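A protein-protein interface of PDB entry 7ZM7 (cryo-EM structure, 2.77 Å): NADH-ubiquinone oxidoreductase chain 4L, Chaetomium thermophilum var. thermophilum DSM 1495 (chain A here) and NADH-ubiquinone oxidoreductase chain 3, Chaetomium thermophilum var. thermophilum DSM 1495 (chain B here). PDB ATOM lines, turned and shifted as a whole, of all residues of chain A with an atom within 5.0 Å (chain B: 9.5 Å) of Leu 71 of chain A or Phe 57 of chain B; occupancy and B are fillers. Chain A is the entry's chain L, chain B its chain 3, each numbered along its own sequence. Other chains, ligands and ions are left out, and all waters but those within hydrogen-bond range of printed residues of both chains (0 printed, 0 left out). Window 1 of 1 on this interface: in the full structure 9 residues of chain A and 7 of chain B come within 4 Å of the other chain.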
ATOM      1  N   LEU A  26       4.894 -22.570  -7.535  1.00  0.00           N
ATOM      2  CA  LEU A  26       4.135 -22.783  -8.760  1.00  0.00           C
ATOM      3  C   LEU A  26       4.679 -21.948  -9.911  1.00  0.00           C
ATOM      4  O   LEU A  26       4.739 -22.412 -11.052  1.00  0.00           O
ATOM      5  CB  LEU A  26       2.670 -22.458  -8.508  1.00  0.00           C
ATOM      6  CG  LEU A  26       1.988 -23.575  -7.747  1.00  0.00           C
ATOM      7  CD1 LEU A  26       0.563 -23.207  -7.435  1.00  0.00           C
ATOM      8  CD2 LEU A  26       2.033 -24.758  -8.643  1.00  0.00           C
ATOM      9  N   GLU A  66      -0.074 -29.059 -16.367  1.00  0.00           N
ATOM     10  CA  GLU A  66       0.383 -29.069 -14.948  1.00  0.00           C
ATOM     11  C   GLU A  66      -0.216 -27.881 -14.206  1.00  0.00           C
ATOM     12  O   GLU A  66      -0.530 -28.045 -13.031  1.00  0.00           O
ATOM     13  CB  GLU A  66       1.894 -29.156 -14.728  1.00  0.00           C
ATOM     14  CG  GLU A  66       2.749 -28.141 -15.445  1.00  0.00           C
ATOM     15  CD  GLU A  66       4.209 -28.553 -15.429  1.00  0.00           C
ATOM     16  OE1 GLU A  66       4.722 -28.945 -16.496  1.00  0.00           O
ATOM     17  OE2 GLU A  66       4.821 -28.509 -14.346  1.00  0.00           O
ATOM     18  N   SER A  67      -0.369 -26.742 -14.876  1.00  0.00           N
ATOM     19  CA  SER A  67      -1.038 -25.601 -14.209  1.00  0.00           C
ATOM     20  C   SER A  67      -2.472 -25.945 -13.781  1.00  0.00           C
ATOM     21  O   SER A  67      -2.826 -25.598 -12.651  1.00  0.00           O
ATOM     22  CB  SER A  67      -1.008 -24.447 -15.126  1.00  0.00           C
ATOM     23  OG  SER A  67       0.313 -24.230 -15.594  1.00  0.00           O
ATOM     24  N   ALA A  68      -3.239 -26.634 -14.624  1.00  0.00           N
ATOM     25  CA  ALA A  68      -4.615 -27.037 -14.263  1.00  0.00           C
ATOM     26  C   ALA A  68      -4.594 -27.987 -13.080  1.00  0.00           C
ATOM     27  O   ALA A  68      -5.373 -27.773 -12.141  1.00  0.00           O
ATOM     28  CB  ALA A  68      -5.260 -27.752 -15.423  1.00  0.00           C
ATOM     29  N   ILE A  69      -3.727 -28.991 -13.134  1.00  0.00           N
ATOM     30  CA  ILE A  69      -3.638 -29.991 -12.033  1.00  0.00           C
ATOM     31  C   ILE A  69      -3.110 -29.280 -10.786  1.00  0.00           C
ATOM     32  O   ILE A  69      -3.628 -29.546  -9.710  1.00  0.00           O
ATOM     33  CB  ILE A  69      -2.791 -31.196 -12.501  1.00  0.00           C
ATOM     34  CG1 ILE A  69      -3.446 -31.921 -13.677  1.00  0.00           C
ATOM     35  CG2 ILE A  69      -2.504 -32.151 -11.354  1.00  0.00           C
ATOM     36  CD1 ILE A  69      -4.826 -32.433 -13.371  1.00  0.00           C
ATOM     37  N   GLY A  70      -2.120 -28.401 -10.947  1.00  0.00           N
ATOM     38  CA  GLY A  70      -1.505 -27.666  -9.831  1.00  0.00           C
ATOM     39  C   GLY A  70      -2.416 -26.671  -9.152  1.00  0.00           C
ATOM     40  O   GLY A  70      -2.335 -26.539  -7.925  1.00  0.00           O
ATOM     41  N   LEU A  71      -3.203 -25.940  -9.944  1.00  0.00           N
ATOM     42  CA  LEU A  71      -4.138 -24.959  -9.363  1.00  0.00           C
ATOM     43  C   LEU A  71      -5.380 -25.711  -8.885  1.00  0.00           C
ATOM     44  O   LEU A  71      -5.986 -25.254  -7.912  1.00  0.00           O
ATOM     45  CB  LEU A  71      -4.425 -23.857 -10.379  1.00  0.00           C
ATOM     46  CG  LEU A  71      -3.297 -22.844 -10.567  1.00  0.00           C
ATOM     47  CD1 LEU A  71      -3.607 -21.888 -11.705  1.00  0.00           C
ATOM     48  CD2 LEU A  71      -3.034 -22.083  -9.278  1.00  0.00           C
ATOM     49  N   GLY A  72      -5.708 -26.843  -9.505  1.00  0.00           N
ATOM     50  CA  GLY A  72      -6.807 -27.627  -8.976  1.00  0.00           C
ATOM     51  C   GLY A  72      -6.512 -28.225  -7.617  1.00  0.00           C
ATOM     52  O   GLY A  72      -7.374 -28.233  -6.735  1.00  0.00           O
ATOM     53  N   ILE A  73      -5.310 -28.771  -7.442  1.00  0.00           N
ATOM     54  CA  ILE A  73      -4.929 -29.348  -6.162  1.00  0.00           C
ATOM     55  C   ILE A  73      -4.779 -28.256  -5.120  1.00  0.00           C
ATOM     56  O   ILE A  73      -5.123 -28.441  -3.948  1.00  0.00           O
ATOM     57  CB  ILE A  73      -3.641 -30.182  -6.321  1.00  0.00           C
ATOM     58  CG1 ILE A  73      -3.947 -31.494  -7.029  1.00  0.00           C
ATOM     59  CG2 ILE A  73      -2.987 -30.491  -4.986  1.00  0.00           C
ATOM     60  CD1 ILE A  73      -2.732 -32.257  -7.429  1.00  0.00           C
ATOM     61  N   LEU A  74      -4.253 -27.103  -5.520  1.00  0.00           N
ATOM     62  CA  LEU A  74      -4.142 -25.989  -4.594  1.00  0.00           C
ATOM     63  C   LEU A  74      -5.510 -25.473  -4.161  1.00  0.00           C
ATOM     64  O   LEU A  74      -5.641 -24.901  -3.079  1.00  0.00           O
ATOM     65  CB  LEU A  74      -3.328 -24.870  -5.223  1.00  0.00           C
ATOM     66  CG  LEU A  74      -3.080 -23.673  -4.327  1.00  0.00           C
ATOM     67  CD1 LEU A  74      -1.842 -23.885  -3.495  1.00  0.00           C
ATOM     68  CD2 LEU A  74      -3.006 -22.410  -5.147  1.00  0.00           C
ATOM     69  N   VAL A  75      -6.528 -25.621  -5.005  1.00  0.00           N
ATOM     70  CA  VAL A  75      -7.877 -25.260  -4.594  1.00  0.00           C
ATOM     71  C   VAL A  75      -8.395 -26.247  -3.564  1.00  0.00           C
ATOM     72  O   VAL A  75      -8.935 -25.858  -2.527  1.00  0.00           O
ATOM     73  CB  VAL A  75      -8.820 -25.183  -5.809  1.00  0.00           C
ATOM     74  CG1 VAL A  75     -10.246 -25.294  -5.352  1.00  0.00           C
ATOM     75  CG2 VAL A  75      -8.617 -23.909  -6.554  1.00  0.00           C
ATOM     76  N   PHE B  52     -14.993 -18.479  -2.145  1.00  0.00           N
ATOM     77  CA  PHE B  52     -15.210 -18.230  -3.559  1.00  0.00           C
ATOM     78  C   PHE B  52     -15.818 -19.462  -4.206  1.00  0.00           C
ATOM     79  O   PHE B  52     -15.577 -20.594  -3.784  1.00  0.00           O
ATOM     80  CB  PHE B  52     -13.907 -17.832  -4.262  1.00  0.00           C
ATOM     81  CG  PHE B  52     -12.967 -18.972  -4.531  1.00  0.00           C
ATOM     82  CD1 PHE B  52     -12.084 -19.391  -3.574  1.00  0.00           C
ATOM     83  CD2 PHE B  52     -12.937 -19.582  -5.764  1.00  0.00           C
ATOM     84  CE1 PHE B  52     -11.218 -20.417  -3.828  1.00  0.00           C
ATOM     85  CE2 PHE B  52     -12.072 -20.619  -6.024  1.00  0.00           C
ATOM     86  CZ  PHE B  52     -11.210 -21.034  -5.060  1.00  0.00           C
ATOM     87  N   ASN B  53     -16.633 -19.223  -5.224  1.00  0.00           N
ATOM     88  CA  ASN B  53     -17.333 -20.303  -5.901  1.00  0.00           C
ATOM     89  C   ASN B  53     -16.375 -21.088  -6.784  1.00  0.00           C
ATOM     90  O   ASN B  53     -15.478 -20.521  -7.411  1.00  0.00           O
ATOM     91  CB  ASN B  53     -18.487 -19.732  -6.714  1.00  0.00           C
ATOM     92  CG  ASN B  53     -19.298 -18.723  -5.919  1.00  0.00           C
ATOM     93  OD1 ASN B  53     -20.051 -19.092  -5.022  1.00  0.00           O
ATOM     94  ND2 ASN B  53     -19.124 -17.437  -6.227  1.00  0.00           N
ATOM     95  N   ILE B  54     -16.554 -22.409  -6.823  1.00  0.00           N
ATOM     96  CA  ILE B  54     -15.603 -23.229  -7.556  1.00  0.00           C
ATOM     97  C   ILE B  54     -15.771 -23.080  -9.059  1.00  0.00           C
ATOM     98  O   ILE B  54     -14.849 -23.393  -9.813  1.00  0.00           O
ATOM     99  CB  ILE B  54     -15.690 -24.704  -7.111  1.00  0.00           C
ATOM    100  CG1 ILE B  54     -14.483 -25.472  -7.635  1.00  0.00           C
ATOM    101  CG2 ILE B  54     -16.945 -25.342  -7.624  1.00  0.00           C
ATOM    102  CD1 ILE B  54     -13.203 -24.950  -7.132  1.00  0.00           C
ATOM    103  N   SER B  55     -16.907 -22.563  -9.511  1.00  0.00           N
ATOM    104  CA  SER B  55     -17.175 -22.490 -10.940  1.00  0.00           C
ATOM    105  C   SER B  55     -16.232 -21.529 -11.648  1.00  0.00           C
ATOM    106  O   SER B  55     -15.982 -21.681 -12.846  1.00  0.00           O
ATOM    107  CB  SER B  55     -18.634 -22.101 -11.173  1.00  0.00           C
ATOM    108  OG  SER B  55     -18.912 -20.819 -10.661  1.00  0.00           O
ATOM    109  N   PHE B  56     -15.691 -20.544 -10.929  1.00  0.00           N
ATOM    110  CA  PHE B  56     -14.658 -19.688 -11.504  1.00  0.00           C
ATOM    111  C   PHE B  56     -13.442 -20.496 -11.919  1.00  0.00           C
ATOM    112  O   PHE B  56     -12.854 -20.254 -12.976  1.00  0.00           O
ATOM    113  CB  PHE B  56     -14.253 -18.613 -10.508  1.00  0.00           C
ATOM    114  CG  PHE B  56     -15.200 -17.475 -10.453  1.00  0.00           C
ATOM    115  CD1 PHE B  56     -15.556 -16.812 -11.611  1.00  0.00           C
ATOM    116  CD2 PHE B  56     -15.744 -17.067  -9.251  1.00  0.00           C
ATOM    117  CE1 PHE B  56     -16.435 -15.778 -11.571  1.00  0.00           C
ATOM    118  CE2 PHE B  56     -16.631 -16.024  -9.207  1.00  0.00           C
ATOM    119  CZ  PHE B  56     -16.970 -15.375 -10.369  1.00  0.00           C
ATOM    120  N   PHE B  57     -13.034 -21.446 -11.085  1.00  0.00           N
ATOM    121  CA  PHE B  57     -11.917 -22.300 -11.442  1.00  0.00           C
ATOM    122  C   PHE B  57     -12.244 -23.130 -12.671  1.00  0.00           C
ATOM    123  O   PHE B  57     -11.405 -23.289 -13.560  1.00  0.00           O
ATOM    124  CB  PHE B  57     -11.539 -23.187 -10.253  1.00  0.00           C
ATOM    125  CG  PHE B  57     -10.506 -24.198 -10.576  1.00  0.00           C
ATOM    126  CD1 PHE B  57      -9.224 -23.806 -10.906  1.00  0.00           C
ATOM    127  CD2 PHE B  57     -10.816 -25.538 -10.594  1.00  0.00           C
ATOM    128  CE1 PHE B  57      -8.271 -24.730 -11.237  1.00  0.00           C
ATOM    129  CE2 PHE B  57      -9.873 -26.461 -10.916  1.00  0.00           C
ATOM    130  CZ  PHE B  57      -8.595 -26.052 -11.240  1.00  0.00           C
ATOM    131  N   ILE B  58     -13.466 -23.648 -12.747  1.00  0.00           N
ATOM    132  CA  ILE B  58     -13.837 -24.536 -13.840  1.00  0.00           C
ATOM    133  C   ILE B  58     -13.879 -23.785 -15.165  1.00  0.00           C
ATOM    134  O   ILE B  58     -13.550 -24.341 -16.212  1.00  0.00           O
ATOM    135  CB  ILE B  58     -15.177 -25.223 -13.527  1.00  0.00           C
ATOM    136  CG1 ILE B  58     -15.184 -25.776 -12.096  1.00  0.00           C
ATOM    137  CG2 ILE B  58     -15.479 -26.304 -14.555  1.00  0.00           C
ATOM    138  CD1 ILE B  58     -14.040 -26.638 -11.754  1.00  0.00           C
ATOM    139  N   TYR B  59     -14.293 -22.522 -15.148  1.00  0.00           N
ATOM    140  CA  TYR B  59     -14.297 -21.731 -16.371  1.00  0.00           C
ATOM    141  C   TYR B  59     -12.896 -21.608 -16.946  1.00  0.00           C
ATOM    142  O   TYR B  59     -12.687 -21.808 -18.145  1.00  0.00           O
ATOM    143  CB  TYR B  59     -14.893 -20.351 -16.095  1.00  0.00           C
ATOM    144  CG  TYR B  59     -16.357 -20.398 -15.776  1.00  0.00           C
ATOM    145  CD1 TYR B  59     -17.126 -21.458 -16.179  1.00  0.00           C
ATOM    146  CD2 TYR B  59     -16.951 -19.428 -14.984  1.00  0.00           C
ATOM    147  CE1 TYR B  59     -18.450 -21.524 -15.875  1.00  0.00           C
ATOM    148  CE2 TYR B  59     -18.280 -19.496 -14.664  1.00  0.00           C
ATOM    149  CZ  TYR B  59     -19.020 -20.547 -15.118  1.00  0.00           C
ATOM    150  OH  TYR B  59     -20.353 -20.640 -14.813  1.00  0.00           O
ATOM    151  N   GLY B  60     -11.919 -21.295 -16.099  1.00  0.00           N
ATOM    152  CA  GLY B  60     -10.554 -21.156 -16.578  1.00  0.00           C
ATOM    153  C   GLY B  60      -9.946 -22.470 -17.029  1.00  0.00           C
ATOM    154  O   GLY B  60      -9.178 -22.510 -17.992  1.00  0.00           O
ATOM    155  N   LEU B  61     -10.270 -23.555 -16.332  1.00  0.00           N
ATOM    156  CA  LEU B  61      -9.690 -24.853 -16.638  1.00  0.00           C
ATOM    157  C   LEU B  61     -10.246 -25.434 -17.930  1.00  0.00           C
ATOM    158  O   LEU B  61      -9.498 -25.944 -18.767  1.00  0.00           O
ATOM    159  CB  LEU B  61      -9.947 -25.792 -15.471  1.00  0.00           C
ATOM    160  CG  LEU B  61      -9.281 -27.154 -15.500  1.00  0.00           C
ATOM    161  CD1 LEU B  61      -9.145 -27.517 -14.108  1.00  0.00           C
ATOM    162  CD2 LEU B  61     -10.119 -28.213 -16.177  1.00  0.00           C
ATOM    163  N   VAL B  62     -11.562 -25.400 -18.092  1.00  0.00           N
ATOM    164  CA  VAL B  62     -12.139 -25.982 -19.288  1.00  0.00           C
ATOM    165  C   VAL B  62     -11.743 -25.173 -20.501  1.00  0.00           C
ATOM    166  O   VAL B  62     -11.537 -25.726 -21.583  1.00  0.00           O
ATOM    167  CB  VAL B  62     -13.657 -26.098 -19.139  1.00  0.00           C
ATOM    168  CG1 VAL B  62     -14.233 -26.743 -20.362  1.00  0.00           C
ATOM    169  CG2 VAL B  62     -13.966 -26.920 -17.928  1.00  0.00           C
ATOM    170  N   PHE B  63     -11.622 -23.859 -20.343  1.00  0.00           N
ATOM    171  CA  PHE B  63     -11.057 -23.032 -21.396  1.00  0.00           C
ATOM    172  C   PHE B  63      -9.614 -23.425 -21.676  1.00  0.00           C
ATOM    173  O   PHE B  63      -9.244 -23.689 -22.820  1.00  0.00           O
ATOM    174  CB  PHE B  63     -11.159 -21.572 -20.981  1.00  0.00           C
ATOM    175  CG  PHE B  63     -10.396 -20.632 -21.836  1.00  0.00           C
ATOM    176  CD1 PHE B  63     -10.669 -20.514 -23.166  1.00  0.00           C
ATOM    177  CD2 PHE B  63      -9.417 -19.850 -21.304  1.00  0.00           C
ATOM    178  CE1 PHE B  63      -9.977 -19.639 -23.952  1.00  0.00           C
ATOM    179  CE2 PHE B  63      -8.722 -18.976 -22.092  1.00  0.00           C
ATOM    180  CZ  PHE B  63      -9.011 -18.865 -23.413  1.00  0.00           C
ATOM    181  N   LEU B  64      -8.798 -23.510 -20.631  1.00  0.00           N
ATOM    182  CA  LEU B  64      -7.375 -23.756 -20.801  1.00  0.00           C
ATOM    183  C   LEU B  64      -7.112 -25.047 -21.559  1.00  0.00           C
ATOM    184  O   LEU B  64      -6.165 -25.134 -22.345  1.00  0.00           O
ATOM    185  CB  LEU B  64      -6.702 -23.801 -19.433  1.00  0.00           C
ATOM    186  CG  LEU B  64      -5.225 -24.149 -19.416  1.00  0.00           C
ATOM    187  CD1 LEU B  64      -4.419 -22.924 -19.698  1.00  0.00           C
ATOM    188  CD2 LEU B  64      -4.838 -24.766 -18.113  1.00  0.00           C
ATOM    189  N   LEU B  65      -7.933 -26.062 -21.341  1.00  0.00           N
ATOM    190  CA  LEU B  65      -7.671 -27.335 -21.985  1.00  0.00           C
ATOM    191  C   LEU B  65      -8.214 -27.357 -23.403  1.00  0.00           C
ATOM    192  O   LEU B  65      -7.482 -27.679 -24.338  1.00  0.00           O
ATOM    193  CB  LEU B  65      -8.246 -28.473 -21.144  1.00  0.00           C
ATOM    194  CG  LEU B  65      -7.592 -28.631 -19.776  1.00  0.00           C
ATOM    195  CD1 LEU B  65      -8.203 -29.795 -19.032  1.00  0.00           C
ATOM    196  CD2 LEU B  65      -6.101 -28.792 -19.893  1.00  0.00           C
ATOM    197  N   GLU B 105     -17.637 -33.440 -18.869  1.00  0.00           N
ATOM    198  CA  GLU B 105     -18.069 -32.239 -18.168  1.00  0.00           C
ATOM    199  C   GLU B 105     -19.498 -31.860 -18.524  1.00  0.00           C
ATOM    200  O   GLU B 105     -20.187 -31.225 -17.723  1.00  0.00           O
ATOM    201  CB  GLU B 105     -17.128 -31.086 -18.459  1.00  0.00           C
ATOM    202  CG  GLU B 105     -17.001 -30.747 -19.902  1.00  0.00           C
ATOM    203  CD  GLU B 105     -15.830 -29.830 -20.151  1.00  0.00           C
ATOM    204  OE1 GLU B 105     -15.237 -29.392 -19.151  1.00  0.00           O
ATOM    205  OE2 GLU B 105     -15.496 -29.559 -21.326  1.00  0.00           O
ATOM    206  N   ALA B 110     -19.894 -29.901 -14.620  1.00  0.00           N
ATOM    207  CA  ALA B 110     -18.745 -29.366 -13.912  1.00  0.00           C
ATOM    208  C   ALA B 110     -18.764 -27.854 -13.946  1.00  0.00           C
ATOM    209  O   ALA B 110     -18.416 -27.196 -12.958  1.00  0.00           O
ATOM    210  CB  ALA B 110     -17.457 -29.913 -14.511  1.00  0.00           C
ATOM    211  N   LEU B 111     -19.204 -27.290 -15.068  1.00  0.00           N
ATOM    212  CA  LEU B 111     -19.355 -25.857 -15.185  1.00  0.00           C
ATOM    213  C   LEU B 111     -20.394 -25.365 -14.190  1.00  0.00           C
ATOM    214  O   LEU B 111     -20.474 -24.162 -13.919  1.00  0.00           O
ATOM    215  CB  LEU B 111     -19.760 -25.511 -16.622  1.00  0.00           C
ATOM    216  CG  LEU B 111     -18.738 -25.423 -17.789  1.00  0.00           C
ATOM    217  CD1 LEU B 111     -17.691 -24.356 -17.657  1.00  0.00           C
ATOM    218  CD2 LEU B 111     -18.072 -26.762 -18.078  1.00  0.00           C
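Ala 68 of chain A touches Phe 57 of chain B. Leu 71 of chain A touches Phe 57 of chain B (C to CE1, 3.9 Å). Gly 72 of chain A touches Phe 57 of chain B (CA to CZ, 3.3 Å). Val 75 of chain A touches Ile 54 of chain B.
Leu 71 of chain A touches just one residue of chain B: Phe 57 (3.9 Å). No residue of chain B comes within 4 Å of Gly 70 of chain A. Printed residues of chain B within 4 Å of Ala 68 of chain A: Phe 57. Of the printed residues of chain B, Val 75 of chain A touches Ile 54. The nearest residue of chain A that does not touch Phe 57 of chain B is Val 75 of chain A (4.4 Å). The nearest printed residue of chain B that does not touch Val 75 of chain A is Phe 52 of chain B (4.1 Å).
Of the 11 printed residues of chain A, 4 touch a printed residue of chain B. Printed residues of chain A that touch a printed residue of chain B: Ala 68, Leu 71, Gly 72 and Val 75. Hydrophobic or aromatic side chains of chain A within 4 Å of the printed part of chain B: Val 75. Hydrophobic or aromatic side chains of chain B that line the printed part of chain A: Ile 54 and Phe 57. Along chain B the printed residues that touch a printed residue of chain A span positions 54 to 57. Among the printed residues, 4 pairs touch across the chains.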
